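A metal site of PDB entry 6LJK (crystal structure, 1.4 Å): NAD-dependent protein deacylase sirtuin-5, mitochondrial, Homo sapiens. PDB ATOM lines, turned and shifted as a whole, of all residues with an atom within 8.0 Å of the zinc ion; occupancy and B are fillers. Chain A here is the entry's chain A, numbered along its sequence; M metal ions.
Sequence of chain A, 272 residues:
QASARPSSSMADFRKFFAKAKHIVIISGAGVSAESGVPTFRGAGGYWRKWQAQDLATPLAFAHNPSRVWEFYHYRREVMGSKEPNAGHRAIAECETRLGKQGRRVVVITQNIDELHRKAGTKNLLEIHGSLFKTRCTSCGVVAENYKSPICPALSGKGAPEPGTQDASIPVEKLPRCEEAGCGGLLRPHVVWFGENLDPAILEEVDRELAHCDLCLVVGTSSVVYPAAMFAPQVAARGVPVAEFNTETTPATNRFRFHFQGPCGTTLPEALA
N of Cys 136 sits at hydrogen-bond distance from O of Val 141, 3.0 Å away. The side-chain sulfur (SG) of Cys 182 lies close to the side-chain hydroxyl (OG) of Ser 138, at 3.8 Å. The side-chain sulfur (SG) of Cys 182 sits close to the backbone NH (N) of Gly 184, 3.5 Å away. The side-chain sulfur of Cys 136 lies close to the backbone NH of Ser 138, at 3.3 Å. N of Cys 177 lies within hydrogen-bond range of O of Gly 184 (2.8 Å). N of Val 141 lies close to SG of Cys 139, at 3.6 Å. The side-chain sulfur of Cys 177 sits close to the backbone NH of Glu 179 (3.5 Å).
Four residues have an atom within 4 Å of the zinc ion: Cys 136, Cys 139, Cys 177 and Cys 182. Along chain A the residues within 4 Å of the zinc ion span positions 136 to 182. The nearest printed residue that does not touch the zinc ion is Val 141 (4.3 Å).
The zinc ion is bound by SG of Cys 182 (2.3 Å), SG of Cys 139 (2.3 Å), SG of Cys 136 (2.4 Å) and SG of Cys 177 (2.4 Å).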
ATOM      1  N   ARG A 135      -7.276   0.300 -29.999  1.00  0.00           N
ATOM      2  CA  ARG A 135      -6.568   0.220 -28.733  1.00  0.00           C
ATOM      3  C   ARG A 135      -5.524   1.333 -28.720  1.00  0.00           C
ATOM      4  O   ARG A 135      -4.823   1.537 -29.716  1.00  0.00           O
ATOM      5  CB  ARG A 135      -5.893  -1.137 -28.518  1.00  0.00           C
ATOM      6  CG  ARG A 135      -5.232  -1.240 -27.176  1.00  0.00           C
ATOM      7  CD  ARG A 135      -4.868  -2.648 -26.812  1.00  0.00           C
ATOM      8  NE  ARG A 135      -3.682  -3.217 -27.481  1.00  0.00           N
ATOM      9  CZ  ARG A 135      -3.694  -4.177 -28.397  1.00  0.00           C
ATOM     10  NH1 ARG A 135      -4.820  -4.647 -28.857  1.00  0.00           N
ATOM     11  NH2 ARG A 135      -2.567  -4.666 -28.859  1.00  0.00           N
ATOM     12  N   CYS A 136      -5.421   2.040 -27.597  1.00  0.00           N
ATOM     13  CA  CYS A 136      -4.416   3.078 -27.482  1.00  0.00           C
ATOM     14  C   CYS A 136      -3.082   2.465 -27.103  1.00  0.00           C
ATOM     15  O   CYS A 136      -2.975   1.738 -26.107  1.00  0.00           O
ATOM     16  CB  CYS A 136      -4.830   4.109 -26.439  1.00  0.00           C
ATOM     17  SG  CYS A 136      -3.616   5.400 -26.255  1.00  0.00           S
ATOM     18  N   THR A 137      -2.051   2.779 -27.876  1.00  0.00           N
ATOM     19  CA  THR A 137      -0.720   2.242 -27.603  1.00  0.00           C
ATOM     20  C   THR A 137      -0.064   2.883 -26.389  1.00  0.00           C
ATOM     21  O   THR A 137       0.970   2.375 -25.947  1.00  0.00           O
ATOM     22  CB  THR A 137       0.204   2.354 -28.831  1.00  0.00           C
ATOM     23  OG1 THR A 137       0.438   3.739 -29.133  1.00  0.00           O
ATOM     24  CG2 THR A 137      -0.382   1.616 -30.030  1.00  0.00           C
ATOM     25  N   SER A 138      -0.624   3.962 -25.844  1.00  0.00           N
ATOM     26  CA  SER A 138      -0.091   4.609 -24.651  1.00  0.00           C
ATOM     27  C   SER A 138      -0.831   4.226 -23.380  1.00  0.00           C
ATOM     28  O   SER A 138      -0.203   3.854 -22.390  1.00  0.00           O
ATOM     29  CB  SER A 138      -0.127   6.135 -24.824  1.00  0.00           C
ATOM     30  OG  SER A 138       0.341   6.794 -23.664  1.00  0.00           O
ATOM     31  N   CYS A 139      -2.164   4.304 -23.362  1.00  0.00           N
ATOM     32  CA  CYS A 139      -2.931   4.020 -22.147  1.00  0.00           C
ATOM     33  C   CYS A 139      -3.635   2.676 -22.166  1.00  0.00           C
ATOM     34  O   CYS A 139      -4.146   2.246 -21.125  1.00  0.00           O
ATOM     35  CB  CYS A 139      -3.952   5.146 -21.857  1.00  0.00           C
ATOM     36  SG  CYS A 139      -5.389   5.142 -22.956  1.00  0.00           S
ATOM     37  N   GLY A 140      -3.678   2.001 -23.307  1.00  0.00           N
ATOM     38  CA  GLY A 140      -4.254   0.674 -23.385  1.00  0.00           C
ATOM     39  C   GLY A 140      -5.757   0.606 -23.532  1.00  0.00           C
ATOM     40  O   GLY A 140      -6.295  -0.498 -23.661  1.00  0.00           O
ATOM     41  N   VAL A 141      -6.467   1.730 -23.523  1.00  0.00           N
ATOM     42  CA  VAL A 141      -7.923   1.667 -23.578  1.00  0.00           C
ATOM     43  C   VAL A 141      -8.375   1.097 -24.913  1.00  0.00           C
ATOM     44  O   VAL A 141      -7.844   1.451 -25.973  1.00  0.00           O
ATOM     45  CB  VAL A 141      -8.570   3.037 -23.348  1.00  0.00           C
ATOM     46  CG1 VAL A 141      -8.203   4.000 -24.428  1.00  0.00           C
ATOM     47  CG2 VAL A 141     -10.089   2.896 -23.289  1.00  0.00           C
ATOM     48  N   VAL A 142      -9.393   0.246 -24.856  1.00  0.00           N
ATOM     49  CA  VAL A 142     -10.033  -0.348 -26.017  1.00  0.00           C
ATOM     50  C   VAL A 142     -11.382   0.320 -26.184  1.00  0.00           C
ATOM     51  O   VAL A 142     -12.148   0.426 -25.224  1.00  0.00           O
ATOM     52  CB  VAL A 142     -10.206  -1.865 -25.816  1.00  0.00           C
ATOM     53  CG1 VAL A 142     -10.982  -2.470 -26.965  1.00  0.00           C
ATOM     54  CG2 VAL A 142      -8.844  -2.512 -25.669  1.00  0.00           C
ATOM     55  N   ARG A 176      -5.759   9.232 -32.955  1.00  0.00           N
ATOM     56  CA  ARG A 176      -5.160   9.501 -31.653  1.00  0.00           C
ATOM     57  C   ARG A 176      -6.192   9.315 -30.555  1.00  0.00           C
ATOM     58  O   ARG A 176      -7.385   9.572 -30.734  1.00  0.00           O
ATOM     59  CB  ARG A 176      -4.596  10.926 -31.554  1.00  0.00           C
ATOM     60  CG  ARG A 176      -3.652  11.335 -32.671  1.00  0.00           C
ATOM     61  CD  ARG A 176      -2.387  10.497 -32.802  1.00  0.00           C
ATOM     62  NE  ARG A 176      -1.530  10.551 -31.601  1.00  0.00           N
ATOM     63  CZ  ARG A 176      -0.229  10.279 -31.599  1.00  0.00           C
ATOM     64  NH1 ARG A 176       0.419   9.969 -32.708  1.00  0.00           N
ATOM     65  NH2 ARG A 176       0.446  10.298 -30.464  1.00  0.00           N
ATOM     66  N   CYS A 177      -5.704   8.897 -29.393  1.00  0.00           N
ATOM     67  CA  CYS A 177      -6.563   8.717 -28.234  1.00  0.00           C
ATOM     68  C   CYS A 177      -7.185  10.034 -27.807  1.00  0.00           C
ATOM     69  O   CYS A 177      -6.510  11.053 -27.750  1.00  0.00           O
ATOM     70  CB  CYS A 177      -5.723   8.154 -27.088  1.00  0.00           C
ATOM     71  SG  CYS A 177      -6.649   7.612 -25.675  1.00  0.00           S
ATOM     72  N   GLU A 178      -8.471   9.997 -27.495  1.00  0.00           N
ATOM     73  CA  GLU A 178      -9.181  11.177 -27.042  1.00  0.00           C
ATOM     74  C   GLU A 178      -9.385  11.207 -25.540  1.00  0.00           C
ATOM     75  O   GLU A 178     -10.027  12.127 -25.036  1.00  0.00           O
ATOM     76  CB  GLU A 178     -10.524  11.301 -27.754  1.00  0.00           C
ATOM     77  CG  GLU A 178     -10.421  11.255 -29.269  1.00  0.00           C
ATOM     78  CD  GLU A 178     -11.783  11.076 -29.903  1.00  0.00           C
ATOM     79  OE1 GLU A 178     -12.107   9.959 -30.392  1.00  0.00           O
ATOM     80  OE2 GLU A 178     -12.545  12.053 -29.905  1.00  0.00           O
ATOM     81  N   GLU A 179      -8.838  10.256 -24.801  1.00  0.00           N
ATOM     82  CA  GLU A 179      -8.896  10.330 -23.349  1.00  0.00           C
ATOM     83  C   GLU A 179      -8.043  11.500 -22.860  1.00  0.00           C
ATOM     84  O   GLU A 179      -6.964  11.764 -23.389  1.00  0.00           O
ATOM     85  CB  GLU A 179      -8.412   9.033 -22.703  1.00  0.00           C
ATOM     86  CG  GLU A 179      -9.212   7.795 -23.100  1.00  0.00           C
ATOM     87  CD  GLU A 179     -10.593   7.701 -22.497  1.00  0.00           C
ATOM     88  OE1 GLU A 179     -10.889   8.421 -21.516  1.00  0.00           O
ATOM     89  OE2 GLU A 179     -11.398   6.895 -22.999  1.00  0.00           O
ATOM     90  N   ALA A 180      -8.539  12.172 -21.840  1.00  0.00           N
ATOM     91  CA  ALA A 180      -7.891  13.391 -21.371  1.00  0.00           C
ATOM     92  C   ALA A 180      -6.441  13.127 -20.985  1.00  0.00           C
ATOM     93  O   ALA A 180      -6.136  12.216 -20.216  1.00  0.00           O
ATOM     94  CB  ALA A 180      -8.658  13.914 -20.154  1.00  0.00           C
ATOM     95  N   GLY A 181      -5.549  13.955 -21.508  1.00  0.00           N
ATOM     96  CA  GLY A 181      -4.147  13.900 -21.154  1.00  0.00           C
ATOM     97  C   GLY A 181      -3.364  12.764 -21.770  1.00  0.00           C
ATOM     98  O   GLY A 181      -2.173  12.634 -21.466  1.00  0.00           O
ATOM     99  N   CYS A 182      -3.970  11.919 -22.603  1.00  0.00           N
ATOM    100  CA  CYS A 182      -3.221  10.797 -23.190  1.00  0.00           C
ATOM    101  C   CYS A 182      -2.597  11.179 -24.532  1.00  0.00           C
ATOM    102  O   CYS A 182      -1.375  11.304 -24.647  1.00  0.00           O
ATOM    103  CB  CYS A 182      -4.126   9.579 -23.320  1.00  0.00           C
ATOM    104  SG  CYS A 182      -3.169   8.173 -23.991  1.00  0.00           S
ATOM    105  N   GLY A 183      -3.422  11.314 -25.566  1.00  0.00           N
ATOM    106  CA  GLY A 183      -2.949  11.688 -26.876  1.00  0.00           C
ATOM    107  C   GLY A 183      -2.194  10.609 -27.617  1.00  0.00           C
ATOM    108  O   GLY A 183      -1.575  10.897 -28.640  1.00  0.00           O
ATOM    109  N   GLY A 184      -2.232   9.364 -27.130  1.00  0.00           N
ATOM    110  CA  GLY A 184      -1.456   8.306 -27.733  1.00  0.00           C
ATOM    111  C   GLY A 184      -1.907   7.940 -29.131  1.00  0.00           C
ATOM    112  O   GLY A 184      -3.031   8.237 -29.562  1.00  0.00           O
ATOM    113  N   LEU A 185      -1.017   7.278 -29.846  1.00  0.00           N
ATOM    114  CA  LEU A 185      -1.340   6.727 -31.144  1.00  0.00           C
ATOM    115  C   LEU A 185      -2.251   5.521 -30.974  1.00  0.00           C
ATOM    116  O   LEU A 185      -1.940   4.589 -30.213  1.00  0.00           O
ATOM    117  CB  LEU A 185      -0.050   6.321 -31.868  1.00  0.00           C
ATOM    118  CG  LEU A 185      -0.209   5.622 -33.222  1.00  0.00           C
ATOM    119  CD1 LEU A 185      -0.932   6.514 -34.250  1.00  0.00           C
ATOM    120  CD2 LEU A 185       1.141   5.174 -33.741  1.00  0.00           C
ATOM    121  N   LEU A 186      -3.373   5.515 -31.674  1.00  0.00           N
ATOM    122  CA  LEU A 186      -4.217   4.328 -31.682  1.00  0.00           C
ATOM    123  C   LEU A 186      -3.736   3.331 -32.729  1.00  0.00           C
ATOM    124  O   LEU A 186      -3.154   3.697 -33.750  1.00  0.00           O
ATOM    125  CB  LEU A 186      -5.672   4.674 -32.005  1.00  0.00           C
ATOM    126  CG  LEU A 186      -6.322   5.722 -31.095  1.00  0.00           C
ATOM    127  CD1 LEU A 186      -7.763   5.970 -31.498  1.00  0.00           C
ATOM    128  CD2 LEU A 186      -6.224   5.291 -29.657  1.00  0.00           C
HETATM  129 ZN    ZN M   1      -4.771   6.641 -24.593  1.00  0.00          ZN
